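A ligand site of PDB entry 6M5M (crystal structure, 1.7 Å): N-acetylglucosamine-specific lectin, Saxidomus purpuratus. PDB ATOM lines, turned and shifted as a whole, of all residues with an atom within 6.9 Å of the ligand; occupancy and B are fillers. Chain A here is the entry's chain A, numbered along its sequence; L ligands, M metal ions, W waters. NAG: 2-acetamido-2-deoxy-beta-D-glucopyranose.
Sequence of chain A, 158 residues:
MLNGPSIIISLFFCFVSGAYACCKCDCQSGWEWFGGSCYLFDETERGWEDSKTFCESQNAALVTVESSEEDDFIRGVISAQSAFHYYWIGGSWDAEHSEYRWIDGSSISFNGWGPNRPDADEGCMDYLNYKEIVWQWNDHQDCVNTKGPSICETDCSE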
ATOM      1  N   HIS A  85      -2.855  -4.150  24.821  1.00  0.00           N
ATOM      2  CA  HIS A  85      -1.588  -4.897  24.681  1.00  0.00           C
ATOM      3  C   HIS A  85      -0.349  -4.095  25.142  1.00  0.00           C
ATOM      4  O   HIS A  85       0.711  -4.684  25.076  1.00  0.00           O
ATOM      5  CB  HIS A  85      -1.399  -5.314  23.233  1.00  0.00           C
ATOM      6  CG  HIS A  85      -2.349  -6.375  22.839  1.00  0.00           C
ATOM      7  ND1 HIS A  85      -3.729  -6.159  22.827  1.00  0.00           N
ATOM      8  CD2 HIS A  85      -2.157  -7.628  22.365  1.00  0.00           C
ATOM      9  CE1 HIS A  85      -4.324  -7.248  22.410  1.00  0.00           C
ATOM     10  NE2 HIS A  85      -3.389  -8.169  22.101  1.00  0.00           N
ATOM     11  N   TYR A  86      -0.484  -2.855  25.579  1.00  0.00           N
ATOM     12  CA  TYR A  86       0.665  -2.062  26.129  1.00  0.00           C
ATOM     13  C   TYR A  86       0.220  -0.941  27.065  1.00  0.00           C
ATOM     14  O   TYR A  86      -0.849  -0.286  26.927  1.00  0.00           O
ATOM     15  CB  TYR A  86       1.590  -1.507  25.019  1.00  0.00           C
ATOM     16  CG  TYR A  86       0.916  -0.613  24.003  1.00  0.00           C
ATOM     17  CD1 TYR A  86       0.827   0.765  24.162  1.00  0.00           C
ATOM     18  CD2 TYR A  86       0.383  -1.122  22.840  1.00  0.00           C
ATOM     19  CE1 TYR A  86       0.257   1.599  23.214  1.00  0.00           C
ATOM     20  CE2 TYR A  86      -0.188  -0.306  21.878  1.00  0.00           C
ATOM     21  CZ  TYR A  86      -0.295   1.067  22.067  1.00  0.00           C
ATOM     22  OH  TYR A  86      -0.898   1.850  21.106  1.00  0.00           O
ATOM     23  N   TRP A  88       2.069   2.368  29.295  1.00  0.00           N
ATOM     24  CA  TRP A  88       3.251   3.236  29.534  1.00  0.00           C
ATOM     25  C   TRP A  88       3.675   3.189  31.005  1.00  0.00           C
ATOM     26  O   TRP A  88       2.846   3.376  31.925  1.00  0.00           O
ATOM     27  CB  TRP A  88       2.959   4.653  29.048  1.00  0.00           C
ATOM     28  CG  TRP A  88       2.753   4.752  27.575  1.00  0.00           C
ATOM     29  CD1 TRP A  88       1.703   5.325  26.936  1.00  0.00           C
ATOM     30  CD2 TRP A  88       3.680   4.382  26.555  1.00  0.00           C
ATOM     31  NE1 TRP A  88       1.884   5.302  25.596  1.00  0.00           N
ATOM     32  CE2 TRP A  88       3.080   4.722  25.324  1.00  0.00           C
ATOM     33  CE3 TRP A  88       4.916   3.764  26.563  1.00  0.00           C
ATOM     34  CZ2 TRP A  88       3.732   4.461  24.122  1.00  0.00           C
ATOM     35  CZ3 TRP A  88       5.584   3.558  25.385  1.00  0.00           C
ATOM     36  CH2 TRP A  88       4.987   3.895  24.178  1.00  0.00           C
ATOM     37  N   ARG A 117      15.271  -6.983  24.701  1.00  0.00           N
ATOM     38  CA  ARG A 117      14.857  -5.581  24.932  1.00  0.00           C
ATOM     39  C   ARG A 117      15.780  -4.971  25.986  1.00  0.00           C
ATOM     40  O   ARG A 117      16.108  -5.669  26.924  1.00  0.00           O
ATOM     41  CB  ARG A 117      13.384  -5.531  25.321  1.00  0.00           C
ATOM     42  CG  ARG A 117      12.459  -6.041  24.229  1.00  0.00           C
ATOM     43  CD  ARG A 117      12.508  -5.180  22.990  1.00  0.00           C
ATOM     44  NE  ARG A 117      11.512  -5.551  22.002  1.00  0.00           N
ATOM     45  CZ  ARG A 117      11.732  -6.425  21.043  1.00  0.00           C
ATOM     46  NH1 ARG A 117      12.900  -7.014  20.956  1.00  0.00           N
ATOM     47  NH2 ARG A 117      10.778  -6.728  20.189  1.00  0.00           N
ATOM     48  N   ASP A 119      15.837  -2.888  22.382  1.00  0.00           N
ATOM     49  CA  ASP A 119      16.426  -3.188  21.039  1.00  0.00           C
ATOM     50  C   ASP A 119      16.935  -1.920  20.364  1.00  0.00           C
ATOM     51  O   ASP A 119      17.458  -2.021  19.243  1.00  0.00           O
ATOM     52  CB  ASP A 119      15.424  -3.935  20.157  1.00  0.00           C
ATOM     53  CG  ASP A 119      14.093  -3.211  19.964  1.00  0.00           C
ATOM     54  OD1 ASP A 119      14.055  -1.991  20.146  1.00  0.00           O
ATOM     55  OD2 ASP A 119      13.118  -3.883  19.639  1.00  0.00           O
ATOM     56  N   CYS A 124      11.054   5.132  25.166  1.00  0.00           N
ATOM     57  CA  CYS A 124      10.323   5.121  26.456  1.00  0.00           C
ATOM     58  C   CYS A 124       9.826   3.690  26.647  1.00  0.00           C
ATOM     59  O   CYS A 124       9.700   2.982  25.641  1.00  0.00           O
ATOM     60  CB  CYS A 124       9.165   6.101  26.476  1.00  0.00           C
ATOM     61  SG  CYS A 124       8.315   6.242  24.894  1.00  0.00           S
ATOM     62  N   ASP A 126       7.274   0.522  28.032  1.00  0.00           N
ATOM     63  CA  ASP A 126       5.883   0.109  28.264  1.00  0.00           C
ATOM     64  C   ASP A 126       5.871  -1.381  28.624  1.00  0.00           C
ATOM     65  O   ASP A 126       6.850  -2.051  28.350  1.00  0.00           O
ATOM     66  CB  ASP A 126       5.003   0.343  27.033  1.00  0.00           C
ATOM     67  CG  ASP A 126       5.477  -0.277  25.741  1.00  0.00           C
ATOM     68  OD1 ASP A 126       6.529  -0.853  25.731  1.00  0.00           O
ATOM     69  OD2 ASP A 126       4.767  -0.165  24.758  1.00  0.00           O
ATOM     70  N   TYR A 127       4.852  -1.799  29.354  1.00  0.00           N
ATOM     71  CA  TYR A 127       4.587  -3.253  29.406  1.00  0.00           C
ATOM     72  C   TYR A 127       3.925  -3.549  28.064  1.00  0.00           C
ATOM     73  O   TYR A 127       3.133  -2.755  27.611  1.00  0.00           O
ATOM     74  CB  TYR A 127       3.718  -3.625  30.613  1.00  0.00           C
ATOM     75  CG  TYR A 127       4.492  -3.897  31.861  1.00  0.00           C
ATOM     76  CD1 TYR A 127       4.976  -5.155  32.156  1.00  0.00           C
ATOM     77  CD2 TYR A 127       4.744  -2.888  32.769  1.00  0.00           C
ATOM     78  CE1 TYR A 127       5.689  -5.413  33.306  1.00  0.00           C
ATOM     79  CE2 TYR A 127       5.445  -3.134  33.934  1.00  0.00           C
ATOM     80  CZ  TYR A 127       5.918  -4.388  34.209  1.00  0.00           C
ATOM     81  OH  TYR A 127       6.617  -4.618  35.348  1.00  0.00           O
ATOM     82  N   LEU A 128       4.298  -4.657  27.461  1.00  0.00           N
ATOM     83  CA  LEU A 128       3.886  -5.109  26.111  1.00  0.00           C
ATOM     84  C   LEU A 128       3.484  -6.582  26.183  1.00  0.00           C
ATOM     85  O   LEU A 128       4.264  -7.417  26.745  1.00  0.00           O
ATOM     86  CB  LEU A 128       5.037  -4.905  25.117  1.00  0.00           C
ATOM     87  CG  LEU A 128       4.732  -5.381  23.696  1.00  0.00           C
ATOM     88  CD1 LEU A 128       3.620  -4.564  23.080  1.00  0.00           C
ATOM     89  CD2 LEU A 128       5.980  -5.335  22.816  1.00  0.00           C
ATOM     90  N   TYR A 130       2.797  -8.959  23.373  1.00  0.00           N
ATOM     91  CA  TYR A 130       2.852  -9.172  21.908  1.00  0.00           C
ATOM     92  C   TYR A 130       4.016 -10.107  21.564  1.00  0.00           C
ATOM     93  O   TYR A 130       5.133  -9.842  22.011  1.00  0.00           O
ATOM     94  CB  TYR A 130       2.962  -7.848  21.160  1.00  0.00           C
ATOM     95  CG  TYR A 130       2.904  -7.907  19.653  1.00  0.00           C
ATOM     96  CD1 TYR A 130       1.922  -8.626  18.977  1.00  0.00           C
ATOM     97  CD2 TYR A 130       3.843  -7.233  18.896  1.00  0.00           C
ATOM     98  CE1 TYR A 130       1.885  -8.676  17.593  1.00  0.00           C
ATOM     99  CE2 TYR A 130       3.793  -7.238  17.513  1.00  0.00           C
ATOM    100  CZ  TYR A 130       2.825  -7.984  16.849  1.00  0.00           C
ATOM    101  OH  TYR A 130       2.821  -8.016  15.491  1.00  0.00           O
ATOM    102  N   LYS A 131       3.724 -11.184  20.825  1.00  0.00           N
ATOM    103  CA  LYS A 131       4.714 -12.222  20.436  1.00  0.00           C
ATOM    104  C   LYS A 131       5.440 -12.727  21.694  1.00  0.00           C
ATOM    105  O   LYS A 131       4.768 -13.117  22.630  1.00  0.00           O
ATOM    106  CB  LYS A 131       5.693 -11.613  19.428  1.00  0.00           C
ATOM    107  CG  LYS A 131       5.056 -10.896  18.250  1.00  0.00           C
ATOM    108  CD  LYS A 131       5.987  -9.857  17.632  1.00  0.00           C
ATOM    109  CE  LYS A 131       6.095  -9.989  16.126  1.00  0.00           C
ATOM    110  NZ  LYS A 131       4.867 -10.534  15.514  1.00  0.00           N
ATOM    111  N   GLU A 132       6.770 -12.574  21.743  1.00  0.00           N
ATOM    112  CA  GLU A 132       7.678 -13.161  22.767  1.00  0.00           C
ATOM    113  C   GLU A 132       7.626 -12.339  24.058  1.00  0.00           C
ATOM    114  O   GLU A 132       8.273 -12.769  25.056  1.00  0.00           O
ATOM    115  CB  GLU A 132       9.144 -13.172  22.316  1.00  0.00           C
ATOM    116  CG  GLU A 132       9.358 -13.446  20.837  1.00  0.00           C
ATOM    117  CD  GLU A 132       8.563 -14.618  20.293  1.00  0.00           C
ATOM    118  OE1 GLU A 132       8.015 -14.490  19.180  1.00  0.00           O
ATOM    119  OE2 GLU A 132       8.495 -15.654  20.984  1.00  0.00           O
ATOM    120  N   ILE A 133       6.963 -11.185  24.049  1.00  0.00           N
ATOM    121  CA  ILE A 133       6.913 -10.283  25.241  1.00  0.00           C
ATOM    122  C   ILE A 133       5.544 -10.463  25.888  1.00  0.00           C
ATOM    123  O   ILE A 133       4.567  -9.886  25.397  1.00  0.00           O
ATOM    124  CB  ILE A 133       7.287  -8.835  24.872  1.00  0.00           C
ATOM    125  CG1 ILE A 133       8.637  -8.797  24.131  1.00  0.00           C
ATOM    126  CG2 ILE A 133       7.305  -7.936  26.113  1.00  0.00           C
ATOM    127  CD1 ILE A 133       8.599  -8.201  22.742  1.00  0.00           C
ATOM    128  N   ASN A 138       9.235  -3.315  27.160  1.00  0.00           N
ATOM    129  CA  ASN A 138       9.740  -3.044  25.803  1.00  0.00           C
ATOM    130  C   ASN A 138      10.094  -1.549  25.743  1.00  0.00           C
ATOM    131  O   ASN A 138       9.602  -0.803  26.571  1.00  0.00           O
ATOM    132  CB  ASN A 138       8.716  -3.483  24.758  1.00  0.00           C
ATOM    133  CG  ASN A 138       8.967  -2.974  23.357  1.00  0.00           C
ATOM    134  OD1 ASN A 138       9.787  -3.532  22.630  1.00  0.00           O
ATOM    135  ND2 ASN A 138       8.252  -1.908  22.983  1.00  0.00           N
ATOM    136  N   ASP A 139      10.999  -1.200  24.844  1.00  0.00           N
ATOM    137  CA  ASP A 139      11.352   0.189  24.464  1.00  0.00           C
ATOM    138  C   ASP A 139      10.671   0.501  23.138  1.00  0.00           C
ATOM    139  O   ASP A 139      10.791  -0.338  22.200  1.00  0.00           O
ATOM    140  CB  ASP A 139      12.867   0.346  24.309  1.00  0.00           C
ATOM    141  CG  ASP A 139      13.458  -0.513  23.206  1.00  0.00           C
ATOM    142  OD1 ASP A 139      13.497  -1.755  23.389  1.00  0.00           O
ATOM    143  OD2 ASP A 139      13.793   0.064  22.152  1.00  0.00           O
ATOM    144  N   HIS A 140       9.953   1.616  23.095  1.00  0.00           N
ATOM    145  CA  HIS A 140       9.280   2.204  21.909  1.00  0.00           C
ATOM    146  C   HIS A 140       9.999   3.516  21.558  1.00  0.00           C
ATOM    147  O   HIS A 140      10.249   4.264  22.499  1.00  0.00           O
ATOM    148  CB  HIS A 140       7.770   2.455  22.206  1.00  0.00           C
ATOM    149  CG  HIS A 140       6.981   2.639  20.947  1.00  0.00           C
ATOM    150  ND1 HIS A 140       6.909   1.603  19.989  1.00  0.00           N
ATOM    151  CD2 HIS A 140       6.306   3.678  20.436  1.00  0.00           C
ATOM    152  CE1 HIS A 140       6.222   2.032  18.968  1.00  0.00           C
ATOM    153  NE2 HIS A 140       5.786   3.266  19.223  1.00  0.00           N
ATOM    154  N   GLN A 141      10.213   3.824  20.283  1.00  0.00           N
ATOM    155  CA  GLN A 141      11.007   5.031  19.880  1.00  0.00           C
ATOM    156  C   GLN A 141      10.101   6.204  19.490  1.00  0.00           C
ATOM    157  O   GLN A 141      10.639   7.231  19.057  1.00  0.00           O
ATOM    158  CB  GLN A 141      11.999   4.662  18.790  1.00  0.00           C
ATOM    159  CG  GLN A 141      13.323   4.099  19.326  1.00  0.00           C
ATOM    160  CD  GLN A 141      13.149   2.930  20.257  1.00  0.00           C
ATOM    161  OE1 GLN A 141      12.514   1.939  19.913  1.00  0.00           O
ATOM    162  NE2 GLN A 141      13.781   2.985  21.415  1.00  0.00           N
ATOM    163  N   ASP A 142       8.774   6.105  19.690  1.00  0.00           N
ATOM    164  CA  ASP A 142       7.837   7.258  19.558  1.00  0.00           C
ATOM    165  C   ASP A 142       7.233   7.528  20.925  1.00  0.00           C
ATOM    166  O   ASP A 142       6.222   6.833  21.354  1.00  0.00           O
ATOM    167  CB  ASP A 142       6.757   7.072  18.487  1.00  0.00           C
ATOM    168  CG  ASP A 142       5.810   8.260  18.347  1.00  0.00           C
ATOM    169  OD1 ASP A 142       5.930   9.240  19.099  1.00  0.00           O
ATOM    170  OD2 ASP A 142       4.935   8.207  17.469  1.00  0.00           O
ATOM    171  N   THR A 146       2.484   7.640  19.973  1.00  0.00           N
ATOM    172  CA  THR A 146       1.893   6.279  20.183  1.00  0.00           C
ATOM    173  C   THR A 146       1.082   6.294  21.489  1.00  0.00           C
ATOM    174  O   THR A 146       1.692   6.401  22.576  1.00  0.00           O
ATOM    175  CB  THR A 146       2.971   5.211  20.127  1.00  0.00           C
ATOM    176  OG1 THR A 146       3.694   5.406  18.909  1.00  0.00           O
ATOM    177  CG2 THR A 146       2.405   3.806  20.110  1.00  0.00           C
ATOM    178  N   LYS A 147      -0.252   6.272  21.370  1.00  0.00           N
ATOM    179  CA  LYS A 147      -1.207   6.414  22.505  1.00  0.00           C
ATOM    180  C   LYS A 147      -1.509   5.043  23.124  1.00  0.00           C
ATOM    181  O   LYS A 147      -1.626   4.010  22.395  1.00  0.00           O
ATOM    182  CB  LYS A 147      -2.489   7.151  22.121  1.00  0.00           C
ATOM    183  CG  LYS A 147      -2.374   8.347  21.183  1.00  0.00           C
ATOM    184  CD  LYS A 147      -3.692   9.076  21.083  1.00  0.00           C
ATOM    185  CE  LYS A 147      -3.700  10.076  19.931  1.00  0.00           C
ATOM    186  NZ  LYS A 147      -4.951  10.840  19.885  1.00  0.00           N
HETATM  187  C1  NAG L   1       5.354  -3.156  18.932  1.00  0.00           C
HETATM  188  C2  NAG L   1       5.669  -2.255  20.106  1.00  0.00           C
HETATM  189  C3  NAG L   1       7.050  -1.919  19.513  1.00  0.00           C
HETATM  190  C4  NAG L   1       7.815  -3.186  19.383  1.00  0.00           C
HETATM  191  C5  NAG L   1       7.062  -4.322  18.684  1.00  0.00           C
HETATM  192  C6  NAG L   1       7.896  -5.568  18.745  1.00  0.00           C
HETATM  193  C7  NAG L   1       4.616  -0.534  21.444  1.00  0.00           C
HETATM  194  C8  NAG L   1       3.728   0.609  21.392  1.00  0.00           C
HETATM  195  N2  NAG L   1       4.763  -1.155  20.246  1.00  0.00           N
HETATM  196  O1  NAG L   1       4.258  -2.915  18.151  1.00  0.00           O
HETATM  197  O3  NAG L   1       7.814  -1.013  20.292  1.00  0.00           O
HETATM  198  O4  NAG L   1       9.061  -3.005  18.656  1.00  0.00           O
HETATM  199  O5  NAG L   1       5.735  -4.454  19.268  1.00  0.00           O
HETATM  200  O6  NAG L   1       7.926  -6.024  20.074  1.00  0.00           O
HETATM  201  O7  NAG L   1       5.157  -0.879  22.492  1.00  0.00           O
HETATM  202 CA    CA M   1      12.213  -0.366  20.381  1.00  0.00          CA
HETATM  203  O   HOH W   1      10.180   0.262  19.180  1.00  0.00           O
HETATM  204  O   HOH W   2       3.248  -4.438  16.261  1.00  0.00           O
HETATM  205  O   HOH W   3      10.984  -2.462  20.485  1.00  0.00           O
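Water W3 lies within hydrogen-bond range of OD1 of Asn 138 (2.7 Å), OD2 of Asp 119 (2.7 Å), O4 of the ligand (2.7 Å) and NE of Arg 117 (3.5 Å).
The side-chain carboxylate of Asp 126 sits close to an oxygen (O7) of the ligand (2.4 Å).
ND1 of His 140 is in hydrogen-bond range of O3 of the ligand (2.8 Å).
O3 of the ligand lies within hydrogen-bond range of ND2 of Asn 138 (2.9 Å).
The guanidinium group (NH2) of Arg 117 is in hydrogen-bond range of an oxygen (O6) of the ligand (2.9 Å).
The backbone carbonyl oxygen (O) of Asp 126 sits at hydrogen-bond distance from the backbone NH (N) of Asn 138 (2.9 Å).
A ring nitrogen (NE2) of His 140 lies within hydrogen-bond range of the side-chain hydroxyl (OG1) of Thr 146 (3.0 Å).
N of His 140 sits at hydrogen-bond distance from O of Cys 124 (2.9 Å).
The guanidinium group (NE) of Arg 117 sits at hydrogen-bond distance from the side-chain amide oxygen (OD1) of Asn 138 (2.7 Å).
The side-chain carboxylate of Asp 119 lies within salt-bridge range of the guanidinium group of Arg 117 (3.3 Å).
The side-chain amino group of Lys 131 is in hydrogen-bond range of the side-chain hydroxyl of Tyr 130, 3.2 Å away.
NE1 of Trp 88 lies close to O of Thr 146 (3.2 Å).
The side-chain hydroxyl of Thr 146 is in hydrogen-bond range of the side-chain carboxylate of Asp 142 (3.4 Å).
Residues that only touch the ligand: Leu 128, Tyr 130, Ile 133, Asp 139 and Thr 146.
Hydrophobic or aromatic side chains that line the ligand: Leu 128, Tyr 130, Ile 133 and His 140.
Nine residues have an atom within 4 Å of the ligand: Arg 117, Asp 126, Leu 128, Tyr 130, Ile 133, Asn 138, Asp 139, His 140 and Thr 146.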
